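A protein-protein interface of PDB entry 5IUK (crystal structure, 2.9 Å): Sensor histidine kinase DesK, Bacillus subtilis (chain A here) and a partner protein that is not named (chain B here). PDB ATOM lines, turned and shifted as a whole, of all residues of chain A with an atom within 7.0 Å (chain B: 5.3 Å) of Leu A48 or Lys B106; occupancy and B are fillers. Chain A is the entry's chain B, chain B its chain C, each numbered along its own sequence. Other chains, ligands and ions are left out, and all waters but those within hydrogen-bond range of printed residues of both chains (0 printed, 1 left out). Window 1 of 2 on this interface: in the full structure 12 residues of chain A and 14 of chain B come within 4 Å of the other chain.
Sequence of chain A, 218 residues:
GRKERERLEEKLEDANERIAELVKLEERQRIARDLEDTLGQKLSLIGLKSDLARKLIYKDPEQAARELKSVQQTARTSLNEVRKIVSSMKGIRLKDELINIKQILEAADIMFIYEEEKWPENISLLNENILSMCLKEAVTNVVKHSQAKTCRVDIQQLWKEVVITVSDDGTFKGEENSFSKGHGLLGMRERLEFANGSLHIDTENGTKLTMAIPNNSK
OE1 of Glu B12 is in salt-bridge range of NZ of Lys B106, 2.9 Å away.
OD1 of Asp B58 lies within salt-bridge range of NZ of Lys B106.
N of Lys B106 sits at hydrogen-bond distance from O of Thr B84, 2.9 Å away.
The side-chain amide nitrogen (NE2) of Gln A41 sits close to the side-chain amino group (NZ) of Lys B106, 3.3 Å away.
Leu B17 touches Gln A41 (CD2 to NE2, 3.9 Å).
Gln A41 touches Thr B85.
Ser A44 touches Thr B85.
Leu A45 touches Leu B17.
CD1 of Leu A48 touches CD2 of Leu B21 (3.95 Å).
Leu B24 touches Leu A48 (CD1 to O, 3.4 Å).
Leu A48 touches Lys B106.
Leu B24 touches Leu A52.
Of the printed residues of chain B, Ser A44 touches Thr B85.
Printed residues of chain B within 4 Å of Leu A48: Leu B21, Leu B24 and Lys B106.
Val A71 touches none of the printed residues of chain B.
Printed residues of chain A within 4 Å of Leu B17: Gln A41 and Leu A45.
Printed residues of chain A within 4 Å of Thr B85: Gln A41 and Ser A44.
Lys B106 touches just these residues of chain A: Gln A41 and Leu A48.
Asp B107 touches none of the printed residues of chain A.
The nearest printed residue of chain B that does not touch Ser A44 is Asp B107 (4.05 Å).
Of the 15 printed residues of chain A, 5 touch a printed residue of chain B.
Printed residues of chain A that touch a printed residue of chain B: Gln A41, Ser A44, Leu A45, Leu A48 and Leu A52.
Hydrophobic or aromatic side chains of chain A that line the printed part of chain B: Leu A45, Leu A48 and Leu A52.
Of the 14 printed residues of chain B, 5 touch a printed residue of chain A.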
ATOM      1  N   GLN A  41     -27.169   3.674  -3.536  1.00  0.00           N
ATOM      2  CA  GLN A  41     -27.798   2.364  -3.407  1.00  0.00           C
ATOM      3  C   GLN A  41     -29.035   2.252  -4.266  1.00  0.00           C
ATOM      4  O   GLN A  41     -29.411   1.139  -4.684  1.00  0.00           O
ATOM      5  CB  GLN A  41     -28.113   2.049  -1.927  1.00  0.00           C
ATOM      6  CG  GLN A  41     -26.885   1.938  -0.975  1.00  0.00           C
ATOM      7  CD  GLN A  41     -25.678   1.133  -1.449  1.00  0.00           C
ATOM      8  OE1 GLN A  41     -24.547   1.652  -1.465  1.00  0.00           O
ATOM      9  NE2 GLN A  41     -25.873  -0.155  -1.801  1.00  0.00           N
ATOM     10  N   LYS A  42     -29.667   3.423  -4.527  1.00  0.00           N
ATOM     11  CA  LYS A  42     -30.911   3.553  -5.298  1.00  0.00           C
ATOM     12  C   LYS A  42     -30.631   3.501  -6.785  1.00  0.00           C
ATOM     13  O   LYS A  42     -31.303   2.751  -7.491  1.00  0.00           O
ATOM     14  CB  LYS A  42     -31.696   4.814  -4.881  1.00  0.00           C
ATOM     15  CG  LYS A  42     -31.857   5.016  -3.357  1.00  0.00           C
ATOM     16  CD  LYS A  42     -33.063   4.314  -2.662  1.00  0.00           C
ATOM     17  CE  LYS A  42     -33.023   2.791  -2.686  1.00  0.00           C
ATOM     18  NZ  LYS A  42     -33.976   2.169  -1.731  1.00  0.00           N
ATOM     19  N   LEU A  43     -29.607   4.265  -7.253  1.00  0.00           N
ATOM     20  CA  LEU A  43     -29.153   4.262  -8.644  1.00  0.00           C
ATOM     21  C   LEU A  43     -28.670   2.831  -9.044  1.00  0.00           C
ATOM     22  O   LEU A  43     -28.721   2.492 -10.223  1.00  0.00           O
ATOM     23  CB  LEU A  43     -28.047   5.307  -8.878  1.00  0.00           C
ATOM     24  CG  LEU A  43     -28.456   6.786  -9.017  1.00  0.00           C
ATOM     25  CD1 LEU A  43     -27.238   7.693  -9.106  1.00  0.00           C
ATOM     26  CD2 LEU A  43     -29.289   7.025 -10.256  1.00  0.00           C
ATOM     27  N   SER A  44     -28.242   1.987  -8.059  1.00  0.00           N
ATOM     28  CA  SER A  44     -27.840   0.602  -8.336  1.00  0.00           C
ATOM     29  C   SER A  44     -29.092  -0.241  -8.485  1.00  0.00           C
ATOM     30  O   SER A  44     -29.193  -1.039  -9.429  1.00  0.00           O
ATOM     31  CB  SER A  44     -26.942   0.039  -7.243  1.00  0.00           C
ATOM     32  OG  SER A  44     -25.648   0.624  -7.257  1.00  0.00           O
ATOM     33  N   LEU A  45     -30.072  -0.031  -7.584  1.00  0.00           N
ATOM     34  CA  LEU A  45     -31.359  -0.720  -7.636  1.00  0.00           C
ATOM     35  C   LEU A  45     -32.033  -0.458  -9.003  1.00  0.00           C
ATOM     36  O   LEU A  45     -32.451  -1.407  -9.679  1.00  0.00           O
ATOM     37  CB  LEU A  45     -32.263  -0.245  -6.483  1.00  0.00           C
ATOM     38  CG  LEU A  45     -33.529  -1.052  -6.233  1.00  0.00           C
ATOM     39  CD1 LEU A  45     -33.204  -2.528  -5.969  1.00  0.00           C
ATOM     40  CD2 LEU A  45     -34.291  -0.490  -5.086  1.00  0.00           C
ATOM     41  N   ILE A  46     -32.050   0.815  -9.444  1.00  0.00           N
ATOM     42  CA  ILE A  46     -32.624   1.193 -10.732  1.00  0.00           C
ATOM     43  C   ILE A  46     -31.989   0.432 -11.867  1.00  0.00           C
ATOM     44  O   ILE A  46     -32.716  -0.193 -12.622  1.00  0.00           O
ATOM     45  CB  ILE A  46     -32.598   2.705 -10.938  1.00  0.00           C
ATOM     46  CG1 ILE A  46     -33.612   3.368  -9.951  1.00  0.00           C
ATOM     47  CG2 ILE A  46     -32.864   3.042 -12.421  1.00  0.00           C
ATOM     48  CD1 ILE A  46     -33.533   4.758  -9.802  1.00  0.00           C
ATOM     49  N   GLY A  47     -30.656   0.415 -11.921  1.00  0.00           N
ATOM     50  CA  GLY A  47     -29.896  -0.276 -12.958  1.00  0.00           C
ATOM     51  C   GLY A  47     -30.294  -1.732 -13.061  1.00  0.00           C
ATOM     52  O   GLY A  47     -30.755  -2.201 -14.117  1.00  0.00           O
ATOM     53  N   LEU A  48     -30.200  -2.419 -11.908  1.00  0.00           N
ATOM     54  CA  LEU A  48     -30.526  -3.824 -11.788  1.00  0.00           C
ATOM     55  C   LEU A  48     -31.952  -4.152 -12.121  1.00  0.00           C
ATOM     56  O   LEU A  48     -32.161  -5.120 -12.849  1.00  0.00           O
ATOM     57  CB  LEU A  48     -30.169  -4.351 -10.420  1.00  0.00           C
ATOM     58  CG  LEU A  48     -28.689  -4.476 -10.104  1.00  0.00           C
ATOM     59  CD1 LEU A  48     -28.517  -4.867  -8.651  1.00  0.00           C
ATOM     60  CD2 LEU A  48     -27.973  -5.464 -11.078  1.00  0.00           C
ATOM     61  N   LYS A  49     -32.931  -3.362 -11.626  1.00  0.00           N
ATOM     62  CA  LYS A  49     -34.352  -3.612 -11.912  1.00  0.00           C
ATOM     63  C   LYS A  49     -34.720  -3.268 -13.347  1.00  0.00           C
ATOM     64  O   LYS A  49     -35.605  -3.915 -13.898  1.00  0.00           O
ATOM     65  CB  LYS A  49     -35.296  -2.933 -10.909  1.00  0.00           C
ATOM     66  CG  LYS A  49     -35.019  -3.272  -9.444  1.00  0.00           C
ATOM     67  CD  LYS A  49     -36.154  -2.845  -8.544  1.00  0.00           C
ATOM     68  CE  LYS A  49     -36.594  -3.996  -7.683  1.00  0.00           C
ATOM     69  NZ  LYS A  49     -37.859  -3.689  -6.974  1.00  0.00           N
ATOM     70  N   SER A  50     -34.024  -2.293 -13.977  1.00  0.00           N
ATOM     71  CA  SER A  50     -34.266  -1.948 -15.389  1.00  0.00           C
ATOM     72  C   SER A  50     -33.838  -3.128 -16.261  1.00  0.00           C
ATOM     73  O   SER A  50     -34.614  -3.582 -17.094  1.00  0.00           O
ATOM     74  CB  SER A  50     -33.482  -0.705 -15.793  1.00  0.00           C
ATOM     75  OG  SER A  50     -34.011   0.428 -15.130  1.00  0.00           O
ATOM     76  N   ASP A  51     -32.614  -3.644 -16.010  1.00  0.00           N
ATOM     77  CA  ASP A  51     -31.964  -4.800 -16.630  1.00  0.00           C
ATOM     78  C   ASP A  51     -32.910  -5.978 -16.600  1.00  0.00           C
ATOM     79  O   ASP A  51     -33.197  -6.539 -17.647  1.00  0.00           O
ATOM     80  CB  ASP A  51     -30.667  -5.162 -15.838  1.00  0.00           C
ATOM     81  CG  ASP A  51     -29.488  -5.654 -16.676  1.00  0.00           C
ATOM     82  OD1 ASP A  51     -29.716  -6.451 -17.634  1.00  0.00           O
ATOM     83  OD2 ASP A  51     -28.335  -5.265 -16.361  1.00  0.00           O
ATOM     84  N   LEU A  52     -33.418  -6.329 -15.403  1.00  0.00           N
ATOM     85  CA  LEU A  52     -34.351  -7.421 -15.188  1.00  0.00           C
ATOM     86  C   LEU A  52     -35.621  -7.161 -15.961  1.00  0.00           C
ATOM     87  O   LEU A  52     -35.978  -7.994 -16.778  1.00  0.00           O
ATOM     88  CB  LEU A  52     -34.624  -7.604 -13.680  1.00  0.00           C
ATOM     89  CG  LEU A  52     -35.711  -8.610 -13.250  1.00  0.00           C
ATOM     90  CD1 LEU A  52     -35.404 -10.025 -13.721  1.00  0.00           C
ATOM     91  CD2 LEU A  52     -35.932  -8.560 -11.755  1.00  0.00           C
ATOM     92  N   ALA A  53     -36.269  -5.989 -15.764  1.00  0.00           N
ATOM     93  CA  ALA A  53     -37.493  -5.627 -16.493  1.00  0.00           C
ATOM     94  C   ALA A  53     -37.362  -5.802 -18.006  1.00  0.00           C
ATOM     95  O   ALA A  53     -38.291  -6.302 -18.619  1.00  0.00           O
ATOM     96  CB  ALA A  53     -37.935  -4.209 -16.151  1.00  0.00           C
ATOM     97  N   GLU A  67     -41.614  -4.056 -11.758  1.00  0.00           N
ATOM     98  CA  GLU A  67     -40.238  -3.589 -11.549  1.00  0.00           C
ATOM     99  C   GLU A  67     -40.105  -2.111 -11.952  1.00  0.00           C
ATOM    100  O   GLU A  67     -39.420  -1.343 -11.271  1.00  0.00           O
ATOM    101  CB  GLU A  67     -39.251  -4.443 -12.385  1.00  0.00           C
ATOM    102  CG  GLU A  67     -39.201  -5.931 -12.045  1.00  0.00           C
ATOM    103  CD  GLU A  67     -38.870  -6.355 -10.620  1.00  0.00           C
ATOM    104  OE1 GLU A  67     -38.044  -5.690  -9.948  1.00  0.00           O
ATOM    105  OE2 GLU A  67     -39.425  -7.393 -10.190  1.00  0.00           O
ATOM    106  N   VAL A  71     -38.861   1.119 -10.056  1.00  0.00           N
ATOM    107  CA  VAL A  71     -37.851   1.989 -10.678  1.00  0.00           C
ATOM    108  C   VAL A  71     -38.329   3.453 -10.606  1.00  0.00           C
ATOM    109  O   VAL A  71     -37.627   4.286 -10.037  1.00  0.00           O
ATOM    110  CB  VAL A  71     -37.487   1.567 -12.134  1.00  0.00           C
ATOM    111  CG1 VAL A  71     -36.679   2.645 -12.829  1.00  0.00           C
ATOM    112  CG2 VAL A  71     -36.722   0.246 -12.172  1.00  0.00           C
ATOM    113  N   GLU B  12     -26.372  -9.942   0.706  1.00  0.00           N
ATOM    114  CA  GLU B  12     -26.658  -8.534   0.433  1.00  0.00           C
ATOM    115  C   GLU B  12     -27.676  -8.061   1.474  1.00  0.00           C
ATOM    116  O   GLU B  12     -28.743  -8.658   1.585  1.00  0.00           O
ATOM    117  CB  GLU B  12     -27.183  -8.393  -1.021  1.00  0.00           C
ATOM    118  CG  GLU B  12     -27.721  -7.027  -1.407  1.00  0.00           C
ATOM    119  CD  GLU B  12     -26.778  -5.867  -1.199  1.00  0.00           C
ATOM    120  OE1 GLU B  12     -25.684  -5.897  -1.805  1.00  0.00           O
ATOM    121  OE2 GLU B  12     -27.128  -4.931  -0.442  1.00  0.00           O
ATOM    122  N   LEU B  17     -32.242  -5.174  -3.530  1.00  0.00           N
ATOM    123  CA  LEU B  17     -31.054  -5.486  -4.330  1.00  0.00           C
ATOM    124  C   LEU B  17     -30.774  -7.000  -4.301  1.00  0.00           C
ATOM    125  O   LEU B  17     -30.426  -7.579  -5.338  1.00  0.00           O
ATOM    126  CB  LEU B  17     -29.837  -4.691  -3.776  1.00  0.00           C
ATOM    127  CG  LEU B  17     -29.829  -3.114  -3.868  1.00  0.00           C
ATOM    128  CD1 LEU B  17     -31.040  -2.429  -3.147  1.00  0.00           C
ATOM    129  CD2 LEU B  17     -28.607  -2.539  -3.215  1.00  0.00           C
ATOM    130  N   ALA B  20     -33.430  -8.644  -6.454  1.00  0.00           N
ATOM    131  CA  ALA B  20     -33.161  -8.338  -7.866  1.00  0.00           C
ATOM    132  C   ALA B  20     -31.990  -9.148  -8.416  1.00  0.00           C
ATOM    133  O   ALA B  20     -32.058  -9.598  -9.563  1.00  0.00           O
ATOM    134  CB  ALA B  20     -32.899  -6.852  -8.057  1.00  0.00           C
ATOM    135  N   LEU B  21     -30.925  -9.359  -7.591  1.00  0.00           N
ATOM    136  CA  LEU B  21     -29.753 -10.136  -8.000  1.00  0.00           C
ATOM    137  C   LEU B  21     -30.106 -11.607  -8.198  1.00  0.00           C
ATOM    138  O   LEU B  21     -29.675 -12.211  -9.189  1.00  0.00           O
ATOM    139  CB  LEU B  21     -28.560  -9.966  -7.038  1.00  0.00           C
ATOM    140  CG  LEU B  21     -27.848  -8.607  -7.058  1.00  0.00           C
ATOM    141  CD1 LEU B  21     -27.068  -8.334  -5.747  1.00  0.00           C
ATOM    142  CD2 LEU B  21     -26.952  -8.474  -8.261  1.00  0.00           C
ATOM    143  N   LEU B  24     -32.064 -11.931 -11.347  1.00  0.00           N
ATOM    144  CA  LEU B  24     -31.184 -11.732 -12.477  1.00  0.00           C
ATOM    145  C   LEU B  24     -30.324 -12.942 -12.795  1.00  0.00           C
ATOM    146  O   LEU B  24     -30.163 -13.273 -13.979  1.00  0.00           O
ATOM    147  CB  LEU B  24     -30.338 -10.467 -12.293  1.00  0.00           C
ATOM    148  CG  LEU B  24     -31.031  -9.258 -12.923  1.00  0.00           C
ATOM    149  CD1 LEU B  24     -30.295  -8.000 -12.622  1.00  0.00           C
ATOM    150  CD2 LEU B  24     -31.287  -9.447 -14.456  1.00  0.00           C
ATOM    151  N   ASP B  58     -21.697  -8.845  -0.713  1.00  0.00           N
ATOM    152  CA  ASP B  58     -21.671  -7.398  -0.532  1.00  0.00           C
ATOM    153  C   ASP B  58     -20.593  -7.118   0.539  1.00  0.00           C
ATOM    154  O   ASP B  58     -20.296  -8.019   1.318  1.00  0.00           O
ATOM    155  CB  ASP B  58     -23.038  -6.950  -0.028  1.00  0.00           C
ATOM    156  CG  ASP B  58     -23.159  -5.474   0.301  1.00  0.00           C
ATOM    157  OD1 ASP B  58     -22.539  -4.634  -0.415  1.00  0.00           O
ATOM    158  OD2 ASP B  58     -23.881  -5.149   1.243  1.00  0.00           O
ATOM    159  N   LEU B  83     -19.266  -7.638  -4.446  1.00  0.00           N
ATOM    160  CA  LEU B  83     -19.952  -6.587  -5.124  1.00  0.00           C
ATOM    161  C   LEU B  83     -19.931  -5.339  -4.200  1.00  0.00           C
ATOM    162  O   LEU B  83     -20.178  -5.422  -2.986  1.00  0.00           O
ATOM    163  CB  LEU B  83     -21.380  -6.984  -5.507  1.00  0.00           C
ATOM    164  CG  LEU B  83     -21.568  -8.043  -6.582  1.00  0.00           C
ATOM    165  CD1 LEU B  83     -22.953  -8.119  -6.975  1.00  0.00           C
ATOM    166  CD2 LEU B  83     -20.789  -7.749  -7.826  1.00  0.00           C
ATOM    167  N   THR B  84     -19.578  -4.191  -4.800  1.00  0.00           N
ATOM    168  CA  THR B  84     -19.580  -2.866  -4.193  1.00  0.00           C
ATOM    169  C   THR B  84     -20.179  -1.804  -5.136  1.00  0.00           C
ATOM    170  O   THR B  84     -20.056  -1.911  -6.359  1.00  0.00           O
ATOM    171  CB  THR B  84     -18.177  -2.482  -3.705  1.00  0.00           C
ATOM    172  OG1 THR B  84     -18.205  -1.254  -2.951  1.00  0.00           O
ATOM    173  CG2 THR B  84     -17.194  -2.370  -4.815  1.00  0.00           C
ATOM    174  N   THR B  85     -20.814  -0.773  -4.559  1.00  0.00           N
ATOM    175  CA  THR B  85     -21.297   0.355  -5.348  1.00  0.00           C
ATOM    176  C   THR B  85     -20.121   1.354  -5.469  1.00  0.00           C
ATOM    177  O   THR B  85     -19.994   2.013  -6.497  1.00  0.00           O
ATOM    178  CB  THR B  85     -22.534   1.043  -4.710  1.00  0.00           C
ATOM    179  OG1 THR B  85     -23.568   0.089  -4.470  1.00  0.00           O
ATOM    180  CG2 THR B  85     -23.104   2.180  -5.583  1.00  0.00           C
ATOM    181  N   LEU B 104     -16.335  -6.732  -8.225  1.00  0.00           N
ATOM    182  CA  LEU B 104     -17.071  -6.044  -9.289  1.00  0.00           C
ATOM    183  C   LEU B 104     -17.954  -4.973  -8.730  1.00  0.00           C
ATOM    184  O   LEU B 104     -18.222  -4.984  -7.528  1.00  0.00           O
ATOM    185  CB  LEU B 104     -17.968  -7.071 -10.053  1.00  0.00           C
ATOM    186  CG  LEU B 104     -17.316  -8.380 -10.507  1.00  0.00           C
ATOM    187  CD1 LEU B 104     -18.353  -9.432 -10.866  1.00  0.00           C
ATOM    188  CD2 LEU B 104     -16.327  -8.127 -11.606  1.00  0.00           C
ATOM    189  N   LEU B 105     -18.489  -4.083  -9.619  1.00  0.00           N
ATOM    190  CA  LEU B 105     -19.474  -3.034  -9.248  1.00  0.00           C
ATOM    191  C   LEU B 105     -20.870  -3.622  -9.266  1.00  0.00           C
ATOM    192  O   LEU B 105     -21.189  -4.423 -10.167  1.00  0.00           O
ATOM    193  CB  LEU B 105     -19.439  -1.764 -10.127  1.00  0.00           C
ATOM    194  CG  LEU B 105     -18.135  -1.016 -10.152  1.00  0.00           C
ATOM    195  CD1 LEU B 105     -17.966  -0.225 -11.435  1.00  0.00           C
ATOM    196  CD2 LEU B 105     -17.913  -0.196  -8.831  1.00  0.00           C
ATOM    197  N   LYS B 106     -21.701  -3.228  -8.282  1.00  0.00           N
ATOM    198  CA  LYS B 106     -23.050  -3.768  -8.158  1.00  0.00           C
ATOM    199  C   LYS B 106     -23.911  -3.433  -9.338  1.00  0.00           C
ATOM    200  O   LYS B 106     -24.851  -4.165  -9.636  1.00  0.00           O
ATOM    201  CB  LYS B 106     -23.702  -3.261  -6.894  1.00  0.00           C
ATOM    202  CG  LYS B 106     -23.424  -4.115  -5.717  1.00  0.00           C
ATOM    203  CD  LYS B 106     -24.395  -3.737  -4.635  1.00  0.00           C
ATOM    204  CE  LYS B 106     -23.731  -3.718  -3.285  1.00  0.00           C
ATOM    205  NZ  LYS B 106     -24.673  -3.240  -2.251  1.00  0.00           N
ATOM    206  N   ASP B 107     -23.590  -2.315 -10.001  1.00  0.00           N
ATOM    207  CA  ASP B 107     -24.369  -1.804 -11.112  1.00  0.00           C
ATOM    208  C   ASP B 107     -23.818  -2.258 -12.442  1.00  0.00           C
ATOM    209  O   ASP B 107     -24.391  -1.876 -13.469  1.00  0.00           O
ATOM    210  CB  ASP B 107     -24.557  -0.276 -11.049  1.00  0.00           C
ATOM    211  CG  ASP B 107     -23.242   0.475 -11.188  1.00  0.00           C
ATOM    212  OD1 ASP B 107     -22.449   0.483 -10.191  1.00  0.00           O
ATOM    213  OD2 ASP B 107     -22.993   1.049 -12.292  1.00  0.00           O
ATOM    214  N   SER B 108     -22.787  -3.148 -12.460  1.00  0.00           N
ATOM    215  CA  SER B 108     -22.284  -3.698 -13.726  1.00  0.00           C
ATOM    216  C   SER B 108     -23.448  -4.465 -14.389  1.00  0.00           C
ATOM    217  O   SER B 108     -24.257  -5.067 -13.660  1.00  0.00           O
ATOM    218  CB  SER B 108     -21.098  -4.629 -13.491  1.00  0.00           C
ATOM    219  OG  SER B 108     -21.426  -5.806 -12.764  1.00  0.00           O
